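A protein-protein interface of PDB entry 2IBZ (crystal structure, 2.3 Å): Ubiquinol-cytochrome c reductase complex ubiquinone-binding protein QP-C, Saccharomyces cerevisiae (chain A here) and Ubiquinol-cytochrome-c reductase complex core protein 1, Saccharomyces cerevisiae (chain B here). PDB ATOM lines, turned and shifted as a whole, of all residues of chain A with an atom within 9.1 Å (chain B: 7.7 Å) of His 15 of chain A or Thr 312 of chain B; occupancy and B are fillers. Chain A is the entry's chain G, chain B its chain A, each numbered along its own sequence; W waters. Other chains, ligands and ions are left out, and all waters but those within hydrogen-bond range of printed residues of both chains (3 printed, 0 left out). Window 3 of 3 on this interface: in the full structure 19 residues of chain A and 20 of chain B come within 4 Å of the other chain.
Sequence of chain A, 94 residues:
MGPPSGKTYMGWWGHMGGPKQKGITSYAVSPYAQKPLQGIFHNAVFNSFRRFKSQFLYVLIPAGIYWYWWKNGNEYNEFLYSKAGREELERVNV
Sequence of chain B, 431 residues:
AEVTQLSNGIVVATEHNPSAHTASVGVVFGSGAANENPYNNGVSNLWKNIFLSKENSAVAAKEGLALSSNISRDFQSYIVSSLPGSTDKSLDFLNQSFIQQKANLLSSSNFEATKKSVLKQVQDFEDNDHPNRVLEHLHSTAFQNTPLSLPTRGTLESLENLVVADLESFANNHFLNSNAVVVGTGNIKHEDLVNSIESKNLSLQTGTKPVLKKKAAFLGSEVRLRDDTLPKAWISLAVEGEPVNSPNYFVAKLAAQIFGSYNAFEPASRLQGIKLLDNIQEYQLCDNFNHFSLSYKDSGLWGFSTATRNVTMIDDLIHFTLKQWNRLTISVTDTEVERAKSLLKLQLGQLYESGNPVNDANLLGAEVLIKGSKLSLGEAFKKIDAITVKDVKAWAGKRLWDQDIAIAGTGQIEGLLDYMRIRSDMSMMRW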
ATOM      1  N   THR A   8     -25.915  19.074 -19.800  1.00  0.00           N
ATOM      2  CA  THR A   8     -26.589  18.846 -21.071  1.00  0.00           C
ATOM      3  C   THR A   8     -27.984  18.262 -20.839  1.00  0.00           C
ATOM      4  O   THR A   8     -28.458  18.182 -19.704  1.00  0.00           O
ATOM      5  CB  THR A   8     -25.775  17.854 -21.941  1.00  0.00           C
ATOM      6  OG1 THR A   8     -25.626  16.607 -21.246  1.00  0.00           O
ATOM      7  CG2 THR A   8     -24.388  18.415 -22.234  1.00  0.00           C
ATOM      8  N   TYR A   9     -28.634  17.839 -21.917  1.00  0.00           N
ATOM      9  CA  TYR A   9     -29.961  17.254 -21.807  1.00  0.00           C
ATOM     10  C   TYR A   9     -29.955  15.750 -22.074  1.00  0.00           C
ATOM     11  O   TYR A   9     -30.995  15.158 -22.342  1.00  0.00           O
ATOM     12  CB  TYR A   9     -30.945  17.989 -22.722  1.00  0.00           C
ATOM     13  CG  TYR A   9     -31.234  19.391 -22.246  1.00  0.00           C
ATOM     14  CD1 TYR A   9     -30.541  20.497 -22.764  1.00  0.00           C
ATOM     15  CD2 TYR A   9     -32.165  19.611 -21.240  1.00  0.00           C
ATOM     16  CE1 TYR A   9     -30.772  21.783 -22.277  1.00  0.00           C
ATOM     17  CE2 TYR A   9     -32.404  20.878 -20.751  1.00  0.00           C
ATOM     18  CZ  TYR A   9     -31.707  21.963 -21.265  1.00  0.00           C
ATOM     19  OH  TYR A   9     -31.951  23.203 -20.717  1.00  0.00           O
ATOM     20  N   MET A  10     -28.765  15.152 -22.045  1.00  0.00           N
ATOM     21  CA  MET A  10     -28.596  13.714 -22.233  1.00  0.00           C
ATOM     22  C   MET A  10     -27.432  13.222 -21.349  1.00  0.00           C
ATOM     23  O   MET A  10     -26.392  13.860 -21.274  1.00  0.00           O
ATOM     24  CB  MET A  10     -28.328  13.355 -23.706  1.00  0.00           C
ATOM     25  CG  MET A  10     -28.209  11.846 -23.925  1.00  0.00           C
ATOM     26  SD  MET A  10     -27.780  11.316 -25.594  1.00  0.00           S
ATOM     27  CE  MET A  10     -26.017  11.671 -25.645  1.00  0.00           C
ATOM     28  N   GLY A  11     -27.654  12.134 -20.621  1.00  0.00           N
ATOM     29  CA  GLY A  11     -26.613  11.568 -19.781  1.00  0.00           C
ATOM     30  C   GLY A  11     -26.094  10.294 -20.431  1.00  0.00           C
ATOM     31  O   GLY A  11     -25.838  10.265 -21.640  1.00  0.00           O
ATOM     32  N   TRP A  12     -25.992   9.221 -19.653  1.00  0.00           N
ATOM     33  CA  TRP A  12     -25.506   7.946 -20.180  1.00  0.00           C
ATOM     34  C   TRP A  12     -26.235   6.840 -19.445  1.00  0.00           C
ATOM     35  O   TRP A  12     -26.962   7.116 -18.509  1.00  0.00           O
ATOM     36  CB  TRP A  12     -23.983   7.819 -19.982  1.00  0.00           C
ATOM     37  CG  TRP A  12     -23.300   6.928 -21.011  1.00  0.00           C
ATOM     38  CD1 TRP A  12     -22.855   5.633 -20.836  1.00  0.00           C
ATOM     39  CD2 TRP A  12     -22.979   7.279 -22.367  1.00  0.00           C
ATOM     40  NE1 TRP A  12     -22.276   5.173 -21.997  1.00  0.00           N
ATOM     41  CE2 TRP A  12     -22.334   6.160 -22.950  1.00  0.00           C
ATOM     42  CE3 TRP A  12     -23.169   8.433 -23.142  1.00  0.00           C
ATOM     43  CZ2 TRP A  12     -21.874   6.164 -24.273  1.00  0.00           C
ATOM     44  CZ3 TRP A  12     -22.710   8.439 -24.461  1.00  0.00           C
ATOM     45  CH2 TRP A  12     -22.068   7.308 -25.010  1.00  0.00           C
ATOM     46  N   TRP A  13     -26.030   5.597 -19.862  1.00  0.00           N
ATOM     47  CA  TRP A  13     -26.674   4.441 -19.234  1.00  0.00           C
ATOM     48  C   TRP A  13     -26.625   4.495 -17.711  1.00  0.00           C
ATOM     49  O   TRP A  13     -25.536   4.549 -17.115  1.00  0.00           O
ATOM     50  CB  TRP A  13     -26.020   3.157 -19.728  1.00  0.00           C
ATOM     51  CG  TRP A  13     -26.083   3.038 -21.209  1.00  0.00           C
ATOM     52  CD1 TRP A  13     -25.052   3.164 -22.081  1.00  0.00           C
ATOM     53  CD2 TRP A  13     -27.248   2.763 -21.994  1.00  0.00           C
ATOM     54  NE1 TRP A  13     -25.497   2.981 -23.368  1.00  0.00           N
ATOM     55  CE2 TRP A  13     -26.841   2.727 -23.345  1.00  0.00           C
ATOM     56  CE3 TRP A  13     -28.599   2.534 -21.684  1.00  0.00           C
ATOM     57  CZ2 TRP A  13     -27.737   2.464 -24.401  1.00  0.00           C
ATOM     58  CZ3 TRP A  13     -29.496   2.271 -22.732  1.00  0.00           C
ATOM     59  CH2 TRP A  13     -29.058   2.236 -24.073  1.00  0.00           C
ATOM     60  N   GLY A  14     -27.807   4.534 -17.092  1.00  0.00           N
ATOM     61  CA  GLY A  14     -27.877   4.610 -15.646  1.00  0.00           C
ATOM     62  C   GLY A  14     -28.214   6.012 -15.160  1.00  0.00           C
ATOM     63  O   GLY A  14     -28.657   6.177 -14.019  1.00  0.00           O
ATOM     64  N   HIS A  15     -27.969   7.023 -15.994  1.00  0.00           N
ATOM     65  CA  HIS A  15     -28.282   8.419 -15.653  1.00  0.00           C
ATOM     66  C   HIS A  15     -28.589   9.201 -16.939  1.00  0.00           C
ATOM     67  O   HIS A  15     -28.003  10.255 -17.206  1.00  0.00           O
ATOM     68  CB  HIS A  15     -27.146   9.066 -14.831  1.00  0.00           C
ATOM     69  CG  HIS A  15     -25.811   9.063 -15.515  1.00  0.00           C
ATOM     70  ND1 HIS A  15     -25.292  10.178 -16.141  1.00  0.00           N
ATOM     71  CD2 HIS A  15     -24.902   8.076 -15.698  1.00  0.00           C
ATOM     72  CE1 HIS A  15     -24.126   9.877 -16.684  1.00  0.00           C
ATOM     73  NE2 HIS A  15     -23.866   8.606 -16.430  1.00  0.00           N
ATOM     74  N   MET A  16     -29.536   8.681 -17.719  1.00  0.00           N
ATOM     75  CA  MET A  16     -29.898   9.276 -19.000  1.00  0.00           C
ATOM     76  C   MET A  16     -30.451  10.683 -18.919  1.00  0.00           C
ATOM     77  O   MET A  16     -30.333  11.450 -19.879  1.00  0.00           O
ATOM     78  CB  MET A  16     -30.872   8.382 -19.762  1.00  0.00           C
ATOM     79  CG  MET A  16     -30.732   8.486 -21.274  1.00  0.00           C
ATOM     80  SD  MET A  16     -29.132   7.875 -21.856  1.00  0.00           S
ATOM     81  CE  MET A  16     -29.398   6.102 -21.752  1.00  0.00           C
ATOM     82  N   GLY A  17     -31.038  11.024 -17.773  1.00  0.00           N
ATOM     83  CA  GLY A  17     -31.597  12.351 -17.600  1.00  0.00           C
ATOM     84  C   GLY A  17     -33.108  12.416 -17.777  1.00  0.00           C
ATOM     85  O   GLY A  17     -33.693  13.503 -17.804  1.00  0.00           O
ATOM     86  N   GLY A  18     -33.733  11.257 -17.953  1.00  0.00           N
ATOM     87  CA  GLY A  18     -35.171  11.211 -18.087  1.00  0.00           C
ATOM     88  C   GLY A  18     -35.798  11.281 -16.708  1.00  0.00           C
ATOM     89  O   GLY A  18     -35.084  11.346 -15.698  1.00  0.00           O
ATOM     90  N   PRO A  19     -37.137  11.302 -16.626  1.00  0.00           N
ATOM     91  CA  PRO A  19     -37.813  11.363 -15.325  1.00  0.00           C
ATOM     92  C   PRO A  19     -37.780   9.962 -14.715  1.00  0.00           C
ATOM     93  O   PRO A  19     -37.556   8.982 -15.437  1.00  0.00           O
ATOM     94  CB  PRO A  19     -39.238  11.758 -15.716  1.00  0.00           C
ATOM     95  CG  PRO A  19     -39.440  10.991 -17.008  1.00  0.00           C
ATOM     96  CD  PRO A  19     -38.117  11.278 -17.732  1.00  0.00           C
ATOM     97  N   LYS A  20     -38.006   9.858 -13.408  1.00  0.00           N
ATOM     98  CA  LYS A  20     -38.009   8.555 -12.742  1.00  0.00           C
ATOM     99  C   LYS A  20     -39.165   7.689 -13.242  1.00  0.00           C
ATOM    100  O   LYS A  20     -40.305   8.116 -13.248  1.00  0.00           O
ATOM    101  CB  LYS A  20     -38.078   8.726 -11.224  1.00  0.00           C
ATOM    102  CG  LYS A  20     -36.959   9.592 -10.668  1.00  0.00           C
ATOM    103  CD  LYS A  20     -36.621   9.252  -9.232  1.00  0.00           C
ATOM    104  CE  LYS A  20     -35.663  10.294  -8.625  1.00  0.00           C
ATOM    105  NZ  LYS A  20     -34.455  10.584  -9.487  1.00  0.00           N
ATOM    106  N   ARG B 226     -38.811  -2.146 -14.434  1.00  0.00           N
ATOM    107  CA  ARG B 226     -38.115  -0.927 -14.043  1.00  0.00           C
ATOM    108  C   ARG B 226     -38.818  -0.150 -12.957  1.00  0.00           C
ATOM    109  O   ARG B 226     -40.025   0.016 -12.998  1.00  0.00           O
ATOM    110  CB  ARG B 226     -37.867   0.002 -15.236  1.00  0.00           C
ATOM    111  CG  ARG B 226     -36.552   0.752 -15.066  1.00  0.00           C
ATOM    112  CD  ARG B 226     -36.593   2.217 -15.419  1.00  0.00           C
ATOM    113  NE  ARG B 226     -36.005   2.463 -16.724  1.00  0.00           N
ATOM    114  CZ  ARG B 226     -35.372   3.575 -17.078  1.00  0.00           C
ATOM    115  NH1 ARG B 226     -34.886   3.660 -18.301  1.00  0.00           N
ATOM    116  NH2 ARG B 226     -35.205   4.585 -16.233  1.00  0.00           N
ATOM    117  N   THR B 308     -27.204  -4.852  -7.077  1.00  0.00           N
ATOM    118  CA  THR B 308     -26.172  -3.813  -7.169  1.00  0.00           C
ATOM    119  C   THR B 308     -26.614  -2.349  -7.036  1.00  0.00           C
ATOM    120  O   THR B 308     -27.711  -1.981  -7.434  1.00  0.00           O
ATOM    121  CB  THR B 308     -25.388  -3.941  -8.501  1.00  0.00           C
ATOM    122  OG1 THR B 308     -24.416  -2.895  -8.577  1.00  0.00           O
ATOM    123  CG2 THR B 308     -26.324  -3.826  -9.700  1.00  0.00           C
ATOM    124  N   ARG B 309     -25.733  -1.522  -6.486  1.00  0.00           N
ATOM    125  CA  ARG B 309     -25.979  -0.088  -6.353  1.00  0.00           C
ATOM    126  C   ARG B 309     -25.133   0.674  -7.389  1.00  0.00           C
ATOM    127  O   ARG B 309     -25.178   1.907  -7.468  1.00  0.00           O
ATOM    128  CB  ARG B 309     -25.616   0.404  -4.953  1.00  0.00           C
ATOM    129  CG  ARG B 309     -26.662   0.103  -3.908  1.00  0.00           C
ATOM    130  CD  ARG B 309     -26.034  -0.387  -2.622  1.00  0.00           C
ATOM    131  NE  ARG B 309     -25.030   0.527  -2.099  1.00  0.00           N
ATOM    132  CZ  ARG B 309     -23.744   0.217  -1.955  1.00  0.00           C
ATOM    133  NH1 ARG B 309     -22.892   1.113  -1.467  1.00  0.00           N
ATOM    134  NH2 ARG B 309     -23.306  -0.983  -2.304  1.00  0.00           N
ATOM    135  N   ASN B 310     -24.323  -0.068  -8.138  1.00  0.00           N
ATOM    136  CA  ASN B 310     -23.475   0.531  -9.147  1.00  0.00           C
ATOM    137  C   ASN B 310     -24.316   0.516 -10.413  1.00  0.00           C
ATOM    138  O   ASN B 310     -24.115  -0.298 -11.327  1.00  0.00           O
ATOM    139  CB  ASN B 310     -22.191  -0.273  -9.316  1.00  0.00           C
ATOM    140  CG  ASN B 310     -21.148   0.466 -10.126  1.00  0.00           C
ATOM    141  OD1 ASN B 310     -19.958   0.174 -10.035  1.00  0.00           O
ATOM    142  ND2 ASN B 310     -21.589   1.426 -10.928  1.00  0.00           N
ATOM    143  N   VAL B 311     -25.228   1.477 -10.479  1.00  0.00           N
ATOM    144  CA  VAL B 311     -26.163   1.537 -11.578  1.00  0.00           C
ATOM    145  C   VAL B 311     -25.676   1.976 -12.947  1.00  0.00           C
ATOM    146  O   VAL B 311     -26.363   1.740 -13.936  1.00  0.00           O
ATOM    147  CB  VAL B 311     -27.441   2.277 -11.159  1.00  0.00           C
ATOM    148  CG1 VAL B 311     -28.079   1.530  -9.991  1.00  0.00           C
ATOM    149  CG2 VAL B 311     -27.134   3.727 -10.797  1.00  0.00           C
ATOM    150  N   THR B 312     -24.468   2.517 -13.020  1.00  0.00           N
ATOM    151  CA  THR B 312     -23.918   2.953 -14.296  1.00  0.00           C
ATOM    152  C   THR B 312     -22.926   1.956 -14.880  1.00  0.00           C
ATOM    153  O   THR B 312     -22.302   2.237 -15.904  1.00  0.00           O
ATOM    154  CB  THR B 312     -23.195   4.301 -14.174  1.00  0.00           C
ATOM    155  OG1 THR B 312     -22.124   4.189 -13.233  1.00  0.00           O
ATOM    156  CG2 THR B 312     -24.153   5.384 -13.728  1.00  0.00           C
ATOM    157  N   MET B 313     -22.758   0.813 -14.216  1.00  0.00           N
ATOM    158  CA  MET B 313     -21.823  -0.204 -14.676  1.00  0.00           C
ATOM    159  C   MET B 313     -22.429  -1.591 -14.738  1.00  0.00           C
ATOM    160  O   MET B 313     -21.719  -2.587 -14.831  1.00  0.00           O
ATOM    161  CB  MET B 313     -20.567  -0.204 -13.809  1.00  0.00           C
ATOM    162  CG  MET B 313     -19.798   1.103 -13.892  1.00  0.00           C
ATOM    163  SD  MET B 313     -18.276   1.173 -12.979  1.00  0.00           S
ATOM    164  CE  MET B 313     -17.182   0.293 -14.129  1.00  0.00           C
ATOM    165  N   ILE B 314     -23.752  -1.651 -14.736  1.00  0.00           N
ATOM    166  CA  ILE B 314     -24.454  -2.919 -14.812  1.00  0.00           C
ATOM    167  C   ILE B 314     -23.986  -3.709 -16.035  1.00  0.00           C
ATOM    168  O   ILE B 314     -23.896  -4.934 -15.975  1.00  0.00           O
ATOM    169  CB  ILE B 314     -25.987  -2.683 -14.859  1.00  0.00           C
ATOM    170  CG1 ILE B 314     -26.458  -2.078 -13.545  1.00  0.00           C
ATOM    171  CG2 ILE B 314     -26.723  -3.937 -15.126  1.00  0.00           C
ATOM    172  CD1 ILE B 314     -27.901  -1.654 -13.574  1.00  0.00           C
ATOM    173  N   ASP B 315     -23.645  -3.020 -17.127  1.00  0.00           N
ATOM    174  CA  ASP B 315     -23.202  -3.719 -18.326  1.00  0.00           C
ATOM    175  C   ASP B 315     -21.882  -4.462 -18.117  1.00  0.00           C
ATOM    176  O   ASP B 315     -21.656  -5.506 -18.731  1.00  0.00           O
ATOM    177  CB  ASP B 315     -23.167  -2.799 -19.570  1.00  0.00           C
ATOM    178  CG  ASP B 315     -22.235  -1.605 -19.414  1.00  0.00           C
ATOM    179  OD1 ASP B 315     -22.437  -0.794 -18.482  1.00  0.00           O
ATOM    180  OD2 ASP B 315     -21.307  -1.462 -20.234  1.00  0.00           O
ATOM    181  N   ASP B 316     -21.027  -3.950 -17.235  1.00  0.00           N
ATOM    182  CA  ASP B 316     -19.767  -4.629 -16.954  1.00  0.00           C
ATOM    183  C   ASP B 316     -20.011  -5.862 -16.084  1.00  0.00           C
ATOM    184  O   ASP B 316     -19.411  -6.916 -16.306  1.00  0.00           O
ATOM    185  CB  ASP B 316     -18.743  -3.683 -16.331  1.00  0.00           C
ATOM    186  CG  ASP B 316     -18.238  -2.631 -17.333  1.00  0.00           C
ATOM    187  OD1 ASP B 316     -18.223  -1.433 -16.991  1.00  0.00           O
ATOM    188  OD2 ASP B 316     -17.880  -3.004 -18.472  1.00  0.00           O
ATOM    189  N   GLN B 412     -33.444   0.105 -10.470  1.00  0.00           N
ATOM    190  CA  GLN B 412     -32.764   0.972 -11.431  1.00  0.00           C
ATOM    191  C   GLN B 412     -32.023   0.188 -12.512  1.00  0.00           C
ATOM    192  O   GLN B 412     -30.793   0.156 -12.519  1.00  0.00           O
ATOM    193  CB  GLN B 412     -31.787   1.899 -10.703  1.00  0.00           C
ATOM    194  CG  GLN B 412     -32.480   2.880  -9.792  1.00  0.00           C
ATOM    195  CD  GLN B 412     -31.527   3.793  -9.079  1.00  0.00           C
ATOM    196  OE1 GLN B 412     -31.512   3.847  -7.849  1.00  0.00           O
ATOM    197  NE2 GLN B 412     -30.740   4.545  -9.841  1.00  0.00           N
ATOM    198  N   GLU B 414     -31.993   0.825 -15.876  1.00  0.00           N
ATOM    199  CA  GLU B 414     -31.823   1.550 -17.131  1.00  0.00           C
ATOM    200  C   GLU B 414     -30.489   1.120 -17.779  1.00  0.00           C
ATOM    201  O   GLU B 414     -30.386   1.009 -18.994  1.00  0.00           O
ATOM    202  CB  GLU B 414     -31.826   3.066 -16.892  1.00  0.00           C
ATOM    203  CG  GLU B 414     -31.593   3.902 -18.150  1.00  0.00           C
ATOM    204  CD  GLU B 414     -31.521   5.384 -17.838  1.00  0.00           C
ATOM    205  OE1 GLU B 414     -30.431   5.870 -17.473  1.00  0.00           O
ATOM    206  OE2 GLU B 414     -32.562   6.065 -17.945  1.00  0.00           O
ATOM    207  N   GLY B 415     -29.499   0.823 -16.943  1.00  0.00           N
ATOM    208  CA  GLY B 415     -28.198   0.411 -17.426  1.00  0.00           C
ATOM    209  C   GLY B 415     -28.083  -1.032 -17.902  1.00  0.00           C
ATOM    210  O   GLY B 415     -27.017  -1.440 -18.373  1.00  0.00           O
HETATM  211  O   HOH W   1     -33.391   8.553 -17.075  1.00  0.00           O
HETATM  212  O   HOH W   2     -22.700   4.581 -17.777  1.00  0.00           O
HETATM  213  O   HOH W   3     -30.647   4.685 -12.634  1.00  0.00           O
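OE1 of Glu 414 of chain B sits at hydrogen-bond distance from N of Gly 14 of chain A (3.0 Å). OE1 of Glu 414 of chain B lies within hydrogen-bond range of N of His 15 of chain A (3.1 Å). OE1 of Glu 414 of chain B sits at hydrogen-bond distance from N of Met 16 of chain A, at 3.0 Å.
NH1 of Arg 226 of chain B is in salt-bridge range of OE2 of Glu 414 of chain B. O of Met 16 of chain A lies within hydrogen-bond range of N of Gly 11 of chain A.
Glu 414 of chain B touches Trp 12 of chain A (OE1 to O, 3.8 Å). Trp 13 of chain A touches Thr 312 of chain B (O to CA, 3.6 Å). Trp 13 of chain A touches Glu 414 of chain B. Val 311 of chain B touches Gly 14 of chain A. CD2 of His 15 of chain A touches CG2 of Thr 312 of chain B, 3.4 Å away.
Of chain B, only Thr 312 (3.4 Å) and Glu 414 (3.1 Å) come within 4 Å of His 15 of chain A. Thr 312 of chain B touches just these residues of chain A: Trp 13 (3.6 Å) and His 15 (3.4 Å). Of the printed residues of chain B, Gly 14 of chain A touches Val 311 and Glu 414. Of chain A, only Gly 14 (3.7 Å) comes within 4 Å of Val 311 of chain B. Printed residues of chain B within 4 Å of Trp 13 of chain A: Thr 312 and Glu 414. Of the printed residues of chain B, Met 16 of chain A touches Glu 414 (3.0 Å). Printed residues of chain B within 4 Å of Trp 12 of chain A: Glu 414. Of the printed residues of chain A, Glu 414 of chain B touches Trp 12 (3.8 Å), Trp 13 (3.6 Å), Gly 14 (3.0 Å), His 15 (3.1 Å) and Met 16 (3.0 Å). Asp 316 of chain B touches none of the printed residues of chain A.
Hydrophobic or aromatic side chains of chain A that line the printed part of chain B: Trp 13, His 15 and Met 16. Along chain A the printed residues that touch a printed residue of chain B span positions 12 to 16.
Water W1 lies within hydrogen-bond range of OE2 of Glu 414 of chain B, N of Gly 18 of chain A and N of Gly 17 of chain A. Water W3 bridges NE2 of Gln 412 of chain B (2.8 Å) and O of Gly 14 of chain A (2.8 Å). Water W2 bridges the backbone carbonyl oxygen of Trp 13 of chain A (2.9 Å) and the backbone carbonyl oxygen of Thr 312 of chain B (3.0 Å).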
